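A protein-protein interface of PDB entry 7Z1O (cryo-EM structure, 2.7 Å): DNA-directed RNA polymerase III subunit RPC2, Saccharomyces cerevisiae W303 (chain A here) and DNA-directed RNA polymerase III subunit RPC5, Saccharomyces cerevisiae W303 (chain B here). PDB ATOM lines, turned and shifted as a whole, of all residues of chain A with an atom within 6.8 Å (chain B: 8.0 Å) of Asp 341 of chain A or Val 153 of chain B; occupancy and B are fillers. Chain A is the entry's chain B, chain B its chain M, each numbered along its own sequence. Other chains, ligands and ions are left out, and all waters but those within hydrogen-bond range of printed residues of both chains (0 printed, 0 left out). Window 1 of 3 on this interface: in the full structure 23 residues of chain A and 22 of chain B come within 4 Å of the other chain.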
ATOM      1  N   GLY A 261      -6.342  24.238 -19.149  1.00  0.00           N
ATOM      2  CA  GLY A 261      -7.197  23.061 -19.186  1.00  0.00           C
ATOM      3  C   GLY A 261      -6.753  22.009 -20.187  1.00  0.00           C
ATOM      4  O   GLY A 261      -7.136  20.843 -20.081  1.00  0.00           O
ATOM      5  N   THR A 336      -9.957  36.487 -15.755  1.00  0.00           N
ATOM      6  CA  THR A 336      -9.772  35.894 -14.443  1.00  0.00           C
ATOM      7  C   THR A 336     -10.626  34.638 -14.326  1.00  0.00           C
ATOM      8  O   THR A 336     -11.652  34.488 -14.996  1.00  0.00           O
ATOM      9  CB  THR A 336     -10.116  36.887 -13.320  1.00  0.00           C
ATOM     10  OG1 THR A 336      -9.712  36.345 -12.057  1.00  0.00           O
ATOM     11  CG2 THR A 336     -11.608  37.194 -13.290  1.00  0.00           C
ATOM     12  N   VAL A 337     -10.169  33.715 -13.484  1.00  0.00           N
ATOM     13  CA  VAL A 337     -10.869  32.461 -13.235  1.00  0.00           C
ATOM     14  C   VAL A 337     -11.145  32.360 -11.741  1.00  0.00           C
ATOM     15  O   VAL A 337     -10.321  32.778 -10.919  1.00  0.00           O
ATOM     16  CB  VAL A 337     -10.078  31.240 -13.741  1.00  0.00           C
ATOM     17  CG1 VAL A 337      -9.910  31.309 -15.248  1.00  0.00           C
ATOM     18  CG2 VAL A 337      -8.721  31.163 -13.084  1.00  0.00           C
ATOM     19  N   GLU A 338     -12.327  31.855 -11.392  1.00  0.00           N
ATOM     20  CA  GLU A 338     -12.728  31.676 -10.004  1.00  0.00           C
ATOM     21  C   GLU A 338     -13.000  30.217  -9.666  1.00  0.00           C
ATOM     22  O   GLU A 338     -13.594  29.933  -8.620  1.00  0.00           O
ATOM     23  CB  GLU A 338     -13.961  32.528  -9.692  1.00  0.00           C
ATOM     24  CG  GLU A 338     -13.877  33.964 -10.192  1.00  0.00           C
ATOM     25  CD  GLU A 338     -14.498  34.145 -11.565  1.00  0.00           C
ATOM     26  OE1 GLU A 338     -14.956  33.140 -12.149  1.00  0.00           O
ATOM     27  OE2 GLU A 338     -14.526  35.291 -12.059  1.00  0.00           O
ATOM     28  N   ALA A 339     -12.583  29.291 -10.519  1.00  0.00           N
ATOM     29  CA  ALA A 339     -12.849  27.873 -10.323  1.00  0.00           C
ATOM     30  C   ALA A 339     -11.677  27.091 -10.908  1.00  0.00           C
ATOM     31  O   ALA A 339     -10.603  27.648 -11.153  1.00  0.00           O
ATOM     32  CB  ALA A 339     -14.202  27.487 -10.945  1.00  0.00           C
ATOM     33  N   LEU A 340     -11.882  25.793 -11.129  1.00  0.00           N
ATOM     34  CA  LEU A 340     -10.825  24.928 -11.633  1.00  0.00           C
ATOM     35  C   LEU A 340     -10.732  24.920 -13.153  1.00  0.00           C
ATOM     36  O   LEU A 340      -9.844  24.255 -13.697  1.00  0.00           O
ATOM     37  CB  LEU A 340     -11.035  23.495 -11.137  1.00  0.00           C
ATOM     38  CG  LEU A 340     -10.737  23.187  -9.669  1.00  0.00           C
ATOM     39  CD1 LEU A 340     -11.968  23.404  -8.802  1.00  0.00           C
ATOM     40  CD2 LEU A 340     -10.218  21.768  -9.519  1.00  0.00           C
ATOM     41  N   ASP A 341     -11.616  25.630 -13.850  1.00  0.00           N
ATOM     42  CA  ASP A 341     -11.669  25.588 -15.306  1.00  0.00           C
ATOM     43  C   ASP A 341     -10.786  26.686 -15.890  1.00  0.00           C
ATOM     44  O   ASP A 341     -10.823  27.832 -15.431  1.00  0.00           O
ATOM     45  CB  ASP A 341     -13.109  25.730 -15.794  1.00  0.00           C
ATOM     46  CG  ASP A 341     -13.301  25.195 -17.198  1.00  0.00           C
ATOM     47  OD1 ASP A 341     -14.139  24.290 -17.381  1.00  0.00           O
ATOM     48  OD2 ASP A 341     -12.616  25.679 -18.121  1.00  0.00           O
ATOM     49  N   PHE A 342      -9.998  26.328 -16.905  1.00  0.00           N
ATOM     50  CA  PHE A 342      -9.052  27.236 -17.544  1.00  0.00           C
ATOM     51  C   PHE A 342      -9.286  27.350 -19.048  1.00  0.00           C
ATOM     52  O   PHE A 342      -8.339  27.612 -19.795  1.00  0.00           O
ATOM     53  CB  PHE A 342      -7.618  26.771 -17.284  1.00  0.00           C
ATOM     54  CG  PHE A 342      -7.129  27.030 -15.888  1.00  0.00           C
ATOM     55  CD1 PHE A 342      -7.044  28.317 -15.394  1.00  0.00           C
ATOM     56  CD2 PHE A 342      -6.746  25.980 -15.073  1.00  0.00           C
ATOM     57  CE1 PHE A 342      -6.584  28.550 -14.112  1.00  0.00           C
ATOM     58  CE2 PHE A 342      -6.288  26.208 -13.789  1.00  0.00           C
ATOM     59  CZ  PHE A 342      -6.208  27.494 -13.310  1.00  0.00           C
ATOM     60  N   ARG A 343     -10.523  27.151 -19.510  1.00  0.00           N
ATOM     61  CA  ARG A 343     -10.770  27.041 -20.947  1.00  0.00           C
ATOM     62  C   ARG A 343     -10.588  28.377 -21.657  1.00  0.00           C
ATOM     63  O   ARG A 343     -10.001  28.436 -22.743  1.00  0.00           O
ATOM     64  CB  ARG A 343     -12.172  26.489 -21.202  1.00  0.00           C
ATOM     65  CG  ARG A 343     -12.365  25.942 -22.604  1.00  0.00           C
ATOM     66  CD  ARG A 343     -11.956  24.483 -22.682  1.00  0.00           C
ATOM     67  NE  ARG A 343     -11.567  24.088 -24.031  1.00  0.00           N
ATOM     68  CZ  ARG A 343     -12.417  23.799 -25.006  1.00  0.00           C
ATOM     69  NH1 ARG A 343     -13.726  23.843 -24.818  1.00  0.00           N
ATOM     70  NH2 ARG A 343     -11.942  23.453 -26.197  1.00  0.00           N
ATOM     71  N   GLU A 344     -11.102  29.461 -21.070  1.00  0.00           N
ATOM     72  CA  GLU A 344     -11.019  30.766 -21.721  1.00  0.00           C
ATOM     73  C   GLU A 344      -9.577  31.247 -21.820  1.00  0.00           C
ATOM     74  O   GLU A 344      -9.158  31.768 -22.863  1.00  0.00           O
ATOM     75  CB  GLU A 344     -11.876  31.780 -20.967  1.00  0.00           C
ATOM     76  CG  GLU A 344     -12.307  32.975 -21.801  1.00  0.00           C
ATOM     77  CD  GLU A 344     -13.547  33.651 -21.253  1.00  0.00           C
ATOM     78  OE1 GLU A 344     -13.439  34.353 -20.225  1.00  0.00           O
ATOM     79  OE2 GLU A 344     -14.632  33.483 -21.850  1.00  0.00           O
ATOM     80  N   LYS A 345      -8.802  31.071 -20.748  1.00  0.00           N
ATOM     81  CA  LYS A 345      -7.391  31.447 -20.763  1.00  0.00           C
ATOM     82  C   LYS A 345      -6.618  30.633 -21.794  1.00  0.00           C
ATOM     83  O   LYS A 345      -5.798  31.174 -22.550  1.00  0.00           O
ATOM     84  CB  LYS A 345      -6.799  31.250 -19.368  1.00  0.00           C
ATOM     85  CG  LYS A 345      -5.393  31.778 -19.195  1.00  0.00           C
ATOM     86  CD  LYS A 345      -5.380  33.287 -19.222  1.00  0.00           C
ATOM     87  CE  LYS A 345      -6.146  33.860 -18.044  1.00  0.00           C
ATOM     88  NZ  LYS A 345      -5.450  33.610 -16.756  1.00  0.00           N
ATOM     89  N   ASP A 540     -21.300  28.031 -26.967  1.00  0.00           N
ATOM     90  CA  ASP A 540     -20.463  28.382 -25.831  1.00  0.00           C
ATOM     91  C   ASP A 540     -19.060  27.811 -26.010  1.00  0.00           C
ATOM     92  O   ASP A 540     -18.860  26.792 -26.675  1.00  0.00           O
ATOM     93  CB  ASP A 540     -21.083  27.873 -24.531  1.00  0.00           C
ATOM     94  CG  ASP A 540     -20.534  28.582 -23.309  1.00  0.00           C
ATOM     95  OD1 ASP A 540     -19.700  29.495 -23.474  1.00  0.00           O
ATOM     96  OD2 ASP A 540     -20.939  28.228 -22.182  1.00  0.00           O
ATOM     97  N   THR A 542     -17.232  26.480 -23.774  1.00  0.00           N
ATOM     98  CA  THR A 542     -16.987  25.341 -22.900  1.00  0.00           C
ATOM     99  C   THR A 542     -17.636  24.052 -23.389  1.00  0.00           C
ATOM    100  O   THR A 542     -17.564  23.041 -22.683  1.00  0.00           O
ATOM    101  CB  THR A 542     -17.478  25.652 -21.484  1.00  0.00           C
ATOM    102  OG1 THR A 542     -18.857  26.036 -21.529  1.00  0.00           O
ATOM    103  CG2 THR A 542     -16.665  26.783 -20.879  1.00  0.00           C
ATOM    104  N   HIS B  86     -26.253  15.157 -16.590  1.00  0.00           N
ATOM    105  CA  HIS B  86     -24.910  15.576 -16.962  1.00  0.00           C
ATOM    106  C   HIS B  86     -24.552  15.028 -18.337  1.00  0.00           C
ATOM    107  O   HIS B  86     -25.055  13.987 -18.767  1.00  0.00           O
ATOM    108  CB  HIS B  86     -23.876  15.103 -15.935  1.00  0.00           C
ATOM    109  CG  HIS B  86     -23.969  15.795 -14.611  1.00  0.00           C
ATOM    110  ND1 HIS B  86     -22.859  16.099 -13.854  1.00  0.00           N
ATOM    111  CD2 HIS B  86     -25.036  16.232 -13.904  1.00  0.00           C
ATOM    112  CE1 HIS B  86     -23.239  16.700 -12.740  1.00  0.00           C
ATOM    113  NE2 HIS B  86     -24.555  16.792 -12.746  1.00  0.00           N
ATOM    114  N   VAL B  87     -23.671  15.746 -19.029  1.00  0.00           N
ATOM    115  CA  VAL B  87     -23.209  15.361 -20.357  1.00  0.00           C
ATOM    116  C   VAL B  87     -21.687  15.368 -20.361  1.00  0.00           C
ATOM    117  O   VAL B  87     -21.065  16.399 -20.079  1.00  0.00           O
ATOM    118  CB  VAL B  87     -23.761  16.296 -21.449  1.00  0.00           C
ATOM    119  CG1 VAL B  87     -22.987  16.125 -22.743  1.00  0.00           C
ATOM    120  CG2 VAL B  87     -25.236  16.024 -21.678  1.00  0.00           C
ATOM    121  N   SER B 116     -17.108  20.440  -5.745  1.00  0.00           N
ATOM    122  CA  SER B 116     -16.076  20.872  -6.679  1.00  0.00           C
ATOM    123  C   SER B 116     -16.366  20.464  -8.118  1.00  0.00           C
ATOM    124  O   SER B 116     -15.714  20.987  -9.029  1.00  0.00           O
ATOM    125  CB  SER B 116     -14.713  20.318  -6.256  1.00  0.00           C
ATOM    126  OG  SER B 116     -13.706  20.702  -7.172  1.00  0.00           O
ATOM    127  N   HIS B 117     -17.323  19.553  -8.332  1.00  0.00           N
ATOM    128  CA  HIS B 117     -17.744  19.103  -9.663  1.00  0.00           C
ATOM    129  C   HIS B 117     -16.580  18.539 -10.476  1.00  0.00           C
ATOM    130  O   HIS B 117     -16.405  18.864 -11.651  1.00  0.00           O
ATOM    131  CB  HIS B 117     -18.452  20.220 -10.432  1.00  0.00           C
ATOM    132  CG  HIS B 117     -19.499  20.931  -9.635  1.00  0.00           C
ATOM    133  ND1 HIS B 117     -20.787  20.458  -9.511  1.00  0.00           N
ATOM    134  CD2 HIS B 117     -19.452  22.083  -8.925  1.00  0.00           C
ATOM    135  CE1 HIS B 117     -21.488  21.285  -8.756  1.00  0.00           C
ATOM    136  NE2 HIS B 117     -20.701  22.280  -8.390  1.00  0.00           N
ATOM    137  N   TRP B 119     -15.245  15.340 -12.139  1.00  0.00           N
ATOM    138  CA  TRP B 119     -15.570  14.007 -12.624  1.00  0.00           C
ATOM    139  C   TRP B 119     -14.298  13.260 -12.995  1.00  0.00           C
ATOM    140  O   TRP B 119     -13.401  13.818 -13.632  1.00  0.00           O
ATOM    141  CB  TRP B 119     -16.488  14.087 -13.842  1.00  0.00           C
ATOM    142  CG  TRP B 119     -17.939  14.098 -13.515  1.00  0.00           C
ATOM    143  CD1 TRP B 119     -18.760  15.184 -13.472  1.00  0.00           C
ATOM    144  CD2 TRP B 119     -18.750  12.967 -13.194  1.00  0.00           C
ATOM    145  NE1 TRP B 119     -20.036  14.798 -13.142  1.00  0.00           N
ATOM    146  CE2 TRP B 119     -20.055  13.441 -12.966  1.00  0.00           C
ATOM    147  CE3 TRP B 119     -18.500  11.596 -13.075  1.00  0.00           C
ATOM    148  CZ2 TRP B 119     -21.106  12.595 -12.627  1.00  0.00           C
ATOM    149  CZ3 TRP B 119     -19.544  10.760 -12.746  1.00  0.00           C
ATOM    150  CH2 TRP B 119     -20.830  11.261 -12.522  1.00  0.00           C
ATOM    151  N   GLY B 150     -12.535  15.806 -15.590  1.00  0.00           N
ATOM    152  CA  GLY B 150     -13.227  16.959 -16.136  1.00  0.00           C
ATOM    153  C   GLY B 150     -13.913  17.743 -15.043  1.00  0.00           C
ATOM    154  O   GLY B 150     -14.066  17.278 -13.912  1.00  0.00           O
ATOM    155  N   VAL B 151     -14.328  18.956 -15.399  1.00  0.00           N
ATOM    156  CA  VAL B 151     -15.043  19.849 -14.493  1.00  0.00           C
ATOM    157  C   VAL B 151     -16.378  20.203 -15.129  1.00  0.00           C
ATOM    158  O   VAL B 151     -16.423  20.651 -16.280  1.00  0.00           O
ATOM    159  CB  VAL B 151     -14.233  21.120 -14.184  1.00  0.00           C
ATOM    160  CG1 VAL B 151     -14.990  22.005 -13.210  1.00  0.00           C
ATOM    161  CG2 VAL B 151     -12.865  20.761 -13.624  1.00  0.00           C
ATOM    162  N   GLY B 152     -17.459  20.002 -14.382  1.00  0.00           N
ATOM    163  CA  GLY B 152     -18.782  20.336 -14.868  1.00  0.00           C
ATOM    164  C   GLY B 152     -19.042  21.827 -14.873  1.00  0.00           C
ATOM    165  O   GLY B 152     -18.974  22.479 -13.827  1.00  0.00           O
ATOM    166  N   VAL B 153     -19.344  22.379 -16.044  1.00  0.00           N
ATOM    167  CA  VAL B 153     -19.588  23.807 -16.206  1.00  0.00           C
ATOM    168  C   VAL B 153     -21.084  24.030 -16.361  1.00  0.00           C
ATOM    169  O   VAL B 153     -21.740  23.361 -17.170  1.00  0.00           O
ATOM    170  CB  VAL B 153     -18.822  24.369 -17.414  1.00  0.00           C
ATOM    171  CG1 VAL B 153     -18.995  25.877 -17.499  1.00  0.00           C
ATOM    172  CG2 VAL B 153     -17.358  24.003 -17.318  1.00  0.00           C
ATOM    173  N   GLU B 154     -21.626  24.964 -15.585  1.00  0.00           N
ATOM    174  CA  GLU B 154     -23.045  25.290 -15.655  1.00  0.00           C
ATOM    175  C   GLU B 154     -23.333  26.008 -16.967  1.00  0.00           C
ATOM    176  O   GLU B 154     -22.953  27.170 -17.147  1.00  0.00           O
ATOM    177  CB  GLU B 154     -23.450  26.150 -14.460  1.00  0.00           C
ATOM    178  CG  GLU B 154     -24.883  26.672 -14.506  1.00  0.00           C
ATOM    179  CD  GLU B 154     -25.907  25.685 -13.965  1.00  0.00           C
ATOM    180  OE1 GLU B 154     -25.642  24.464 -13.967  1.00  0.00           O
ATOM    181  OE2 GLU B 154     -26.989  26.137 -13.534  1.00  0.00           O
ATOM    182  N   ASN B 155     -23.998  25.317 -17.888  1.00  0.00           N
ATOM    183  CA  ASN B 155     -24.375  25.875 -19.180  1.00  0.00           C
ATOM    184  C   ASN B 155     -25.888  26.018 -19.215  1.00  0.00           C
ATOM    185  O   ASN B 155     -26.612  25.041 -19.000  1.00  0.00           O
ATOM    186  CB  ASN B 155     -23.887  24.989 -20.325  1.00  0.00           C
ATOM    187  CG  ASN B 155     -22.451  25.271 -20.706  1.00  0.00           C
ATOM    188  OD1 ASN B 155     -21.584  24.407 -20.589  1.00  0.00           O
ATOM    189  ND2 ASN B 155     -22.191  26.488 -21.164  1.00  0.00           N
ATOM    190  N   ASN B 156     -26.360  27.229 -19.488  1.00  0.00           N
ATOM    191  CA  ASN B 156     -27.783  27.531 -19.485  1.00  0.00           C
ATOM    192  C   ASN B 156     -28.338  27.461 -20.901  1.00  0.00           C
ATOM    193  O   ASN B 156     -27.688  27.895 -21.857  1.00  0.00           O
ATOM    194  CB  ASN B 156     -28.045  28.912 -18.888  1.00  0.00           C
ATOM    195  CG  ASN B 156     -28.166  28.880 -17.378  1.00  0.00           C
ATOM    196  OD1 ASN B 156     -29.178  28.437 -16.835  1.00  0.00           O
ATOM    197  ND2 ASN B 156     -27.131  29.349 -16.692  1.00  0.00           N
ATOM    198  N   GLN B 158     -29.346  24.499 -22.403  1.00  0.00           N
ATOM    199  CA  GLN B 158     -29.036  23.225 -23.033  1.00  0.00           C
ATOM    200  C   GLN B 158     -30.034  22.170 -22.577  1.00  0.00           C
ATOM    201  O   GLN B 158     -30.286  22.025 -21.376  1.00  0.00           O
ATOM    202  CB  GLN B 158     -27.611  22.785 -22.701  1.00  0.00           C
ATOM    203  CG  GLN B 158     -26.563  23.829 -23.021  1.00  0.00           C
ATOM    204  CD  GLN B 158     -25.999  23.672 -24.416  1.00  0.00           C
ATOM    205  OE1 GLN B 158     -25.819  22.556 -24.901  1.00  0.00           O
ATOM    206  NE2 GLN B 158     -25.726  24.792 -25.073  1.00  0.00           N
ATOM    207  N   ILE B 173     -30.095  20.021 -19.099  1.00  0.00           N
ATOM    208  CA  ILE B 173     -28.756  19.515 -18.826  1.00  0.00           C
ATOM    209  C   ILE B 173     -28.118  20.422 -17.787  1.00  0.00           C
ATOM    210  O   ILE B 173     -27.990  21.633 -18.003  1.00  0.00           O
ATOM    211  CB  ILE B 173     -27.906  19.450 -20.103  1.00  0.00           C
ATOM    212  CG1 ILE B 173     -28.519  18.468 -21.100  1.00  0.00           C
ATOM    213  CG2 ILE B 173     -26.481  19.053 -19.772  1.00  0.00           C
ATOM    214  CD1 ILE B 173     -27.899  18.534 -22.475  1.00  0.00           C
ATOM    215  N   GLU B 174     -27.719  19.840 -16.655  1.00  0.00           N
ATOM    216  CA  GLU B 174     -27.172  20.641 -15.568  1.00  0.00           C
ATOM    217  C   GLU B 174     -25.768  21.129 -15.894  1.00  0.00           C
ATOM    218  O   GLU B 174     -25.529  22.338 -15.999  1.00  0.00           O
ATOM    219  CB  GLU B 174     -27.174  19.830 -14.272  1.00  0.00           C
ATOM    220  CG  GLU B 174     -27.236  20.672 -13.011  1.00  0.00           C
ATOM    221  CD  GLU B 174     -26.931  19.869 -11.763  1.00  0.00           C
ATOM    222  OE1 GLU B 174     -26.736  18.640 -11.878  1.00  0.00           O
ATOM    223  OE2 GLU B 174     -26.885  20.465 -10.667  1.00  0.00           O
ATOM    224  N   ARG B 175     -24.823  20.206 -16.060  1.00  0.00           N
ATOM    225  CA  ARG B 175     -23.437  20.570 -16.307  1.00  0.00           C
ATOM    226  C   ARG B 175     -22.902  19.752 -17.471  1.00  0.00           C
ATOM    227  O   ARG B 175     -23.382  18.653 -17.759  1.00  0.00           O
ATOM    228  CB  ARG B 175     -22.554  20.355 -15.068  1.00  0.00           C
ATOM    229  CG  ARG B 175     -23.238  20.624 -13.737  1.00  0.00           C
ATOM    230  CD  ARG B 175     -22.258  20.573 -12.583  1.00  0.00           C
ATOM    231  NE  ARG B 175     -21.682  21.883 -12.302  1.00  0.00           N
ATOM    232  CZ  ARG B 175     -22.292  22.842 -11.620  1.00  0.00           C
ATOM    233  NH1 ARG B 175     -23.507  22.672 -11.124  1.00  0.00           N
ATOM    234  NH2 ARG B 175     -21.668  24.000 -11.429  1.00  0.00           N
ATOM    235  N   VAL B 176     -21.896  20.308 -18.141  1.00  0.00           N
ATOM    236  CA  VAL B 176     -21.197  19.643 -19.232  1.00  0.00           C
ATOM    237  C   VAL B 176     -19.731  19.524 -18.843  1.00  0.00           C
ATOM    238  O   VAL B 176     -19.088  20.527 -18.517  1.00  0.00           O
ATOM    239  CB  VAL B 176     -21.346  20.405 -20.562  1.00  0.00           C
ATOM    240  CG1 VAL B 176     -20.531  19.736 -21.652  1.00  0.00           C
ATOM    241  CG2 VAL B 176     -22.807  20.485 -20.963  1.00  0.00           C
ATOM    242  N   ALA B 177     -19.206  18.303 -18.878  1.00  0.00           N
ATOM    243  CA  ALA B 177     -17.841  18.024 -18.457  1.00  0.00           C
ATOM    244  C   ALA B 177     -16.961  17.762 -19.670  1.00  0.00           C
ATOM    245  O   ALA B 177     -17.364  17.056 -20.598  1.00  0.00           O
ATOM    246  CB  ALA B 177     -17.795  16.823 -17.510  1.00  0.00           C
ATOM    247  N   GLN B 178     -15.769  18.354 -19.667  1.00  0.00           N
ATOM    248  CA  GLN B 178     -14.771  18.154 -20.719  1.00  0.00           C
ATOM    249  C   GLN B 178     -13.746  17.159 -20.188  1.00  0.00           C
ATOM    250  O   GLN B 178     -12.740  17.540 -19.586  1.00  0.00           O
ATOM    251  CB  GLN B 178     -14.114  19.474 -21.109  1.00  0.00           C
ATOM    252  CG  GLN B 178     -15.058  20.537 -21.640  1.00  0.00           C
ATOM    253  CD  GLN B 178     -15.383  20.354 -23.106  1.00  0.00           C
ATOM    254  OE1 GLN B 178     -14.524  19.984 -23.904  1.00  0.00           O
ATOM    255  NE2 GLN B 178     -16.629  20.628 -23.473  1.00  0.00           N
ATOM    256  N   LYS B 180     -10.718  15.010 -20.033  1.00  0.00           N
ATOM    257  CA  LYS B 180      -9.410  15.019 -20.664  1.00  0.00           C
ATOM    258  C   LYS B 180      -8.500  14.055 -19.922  1.00  0.00           C
ATOM    259  O   LYS B 180      -8.714  13.786 -18.736  1.00  0.00           O
ATOM    260  CB  LYS B 180      -8.814  16.434 -20.665  1.00  0.00           C
ATOM    261  CG  LYS B 180      -9.623  17.418 -21.489  1.00  0.00           C
ATOM    262  CD  LYS B 180      -8.877  18.714 -21.710  1.00  0.00           C
ATOM    263  CE  LYS B 180      -9.758  19.738 -22.400  1.00  0.00           C
ATOM    264  NZ  LYS B 180     -10.268  19.235 -23.703  1.00  0.00           N
ATOM    265  N   SER B 230      -9.033  31.085  -7.186  1.00  0.00           N
ATOM    266  CA  SER B 230      -8.625  29.802  -7.749  1.00  0.00           C
ATOM    267  C   SER B 230      -7.856  28.964  -6.737  1.00  0.00           C
ATOM    268  O   SER B 230      -7.957  27.731  -6.744  1.00  0.00           O
ATOM    269  CB  SER B 230      -7.785  30.026  -9.005  1.00  0.00           C
ATOM    270  OG  SER B 230      -7.444  28.792  -9.612  1.00  0.00           O
ATOM    271  N   ALA B 233     -10.323  27.254  -4.428  1.00  0.00           N
ATOM    272  CA  ALA B 233     -11.000  26.182  -5.151  1.00  0.00           C
ATOM    273  C   ALA B 233     -10.097  24.966  -5.314  1.00  0.00           C
ATOM    274  O   ALA B 233     -10.538  23.828  -5.121  1.00  0.00           O
ATOM    275  CB  ALA B 233     -11.475  26.685  -6.513  1.00  0.00           C
ATOM    276  N   HIS B 234      -8.825  25.189  -5.653  1.00  0.00           N
ATOM    277  CA  HIS B 234      -7.893  24.075  -5.798  1.00  0.00           C
ATOM    278  C   HIS B 234      -7.648  23.376  -4.465  1.00  0.00           C
ATOM    279  O   HIS B 234      -7.581  22.142  -4.408  1.00  0.00           O
ATOM    280  CB  HIS B 234      -6.577  24.569  -6.398  1.00  0.00           C
ATOM    281  CG  HIS B 234      -6.535  24.502  -7.892  1.00  0.00           C
ATOM    282  ND1 HIS B 234      -6.910  25.557  -8.696  1.00  0.00           N
ATOM    283  CD2 HIS B 234      -6.165  23.505  -8.729  1.00  0.00           C
ATOM    284  CE1 HIS B 234      -6.771  25.212  -9.964  1.00  0.00           C
ATOM    285  NE2 HIS B 234      -6.320  23.972 -10.012  1.00  0.00           N
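The side-chain hydroxyl (OG1) of Thr 542 of chain A lies within hydrogen-bond range of the side-chain amide oxygen (OD1) of Asn 155 of chain B. NE2 of Gln 178 of chain B sits at hydrogen-bond distance from O of Thr 542 of chain A (2.7 Å). OD2 of Asp 540 of chain A lies close to ND2 of Asn 155 of chain B.
The backbone NH of Val 153 of chain B sits at hydrogen-bond distance from the backbone carbonyl oxygen of Val 176 of chain B, 3.1 Å away. The backbone carbonyl oxygen (O) of Ser 230 of chain B is in hydrogen-bond range of a ring nitrogen (ND1) of His 234 of chain B, 3.1 Å away. N of Arg 343 of chain A sits at hydrogen-bond distance from OD2 of Asp 341 of chain A (2.9 Å). OG1 of Thr 542 of chain A sits at hydrogen-bond distance from OD2 of Asp 540 of chain A, 3.1 Å away.
Gly 261 of chain A touches Lys 180 of chain B. O of Ala 339 of chain A touches OG of Ser 230 of chain B, at 3.7 Å. Leu 340 of chain A touches Ser 116 of chain B (CD1 to OG, 3.6 Å). O of Ala 233 of chain B touches CD1 of Leu 340 of chain A, 3.97 Å away. Asp 341 of chain A touches Val 153 of chain B (OD1 to CG2, 3.2 Å). His 234 of chain B touches Phe 342 of chain A (CE1 to CE2, 3.98 Å).
Of chain B, only Val 153 comes within 4 Å of Asp 341 of chain A. Of chain A, only Asp 341 comes within 4 Å of Val 153 of chain B. Of the printed residues of chain A, Gln 178 of chain B touches Thr 542 (2.7 Å). Printed residues of chain A within 4 Å of His 234 of chain B: Phe 342 (3.98 Å). Of the printed residues of chain B, Thr 542 of chain A touches Asn 155 (3.3 Å) and Gln 178 (2.7 Å). Of the printed residues of chain A, Ser 230 of chain B touches Ala 339. Of the printed residues of chain B, Phe 342 of chain A touches His 234 (3.98 Å). His 117 of chain B touches none of the printed residues of chain A. Val 151 of chain B touches none of the printed residues of chain A. The nearest residue of chain B that does not touch Asp 341 of chain A is Val 151 of chain B (4.4 Å).
Of the 23 printed residues of chain B, 8 touch a printed residue of chain A. Printed residues of chain B that touch a printed residue of chain A: Ser 116, Val 153, Asn 155, Gln 178, Lys 180, Ser 230, Ala 233 and His 234. Hydrophobic or aromatic side chains of chain B that line the printed part of chain A: Val 153 and His 234. Along chain A the printed residues that touch a printed residue of chain B span positions 261 to 542.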
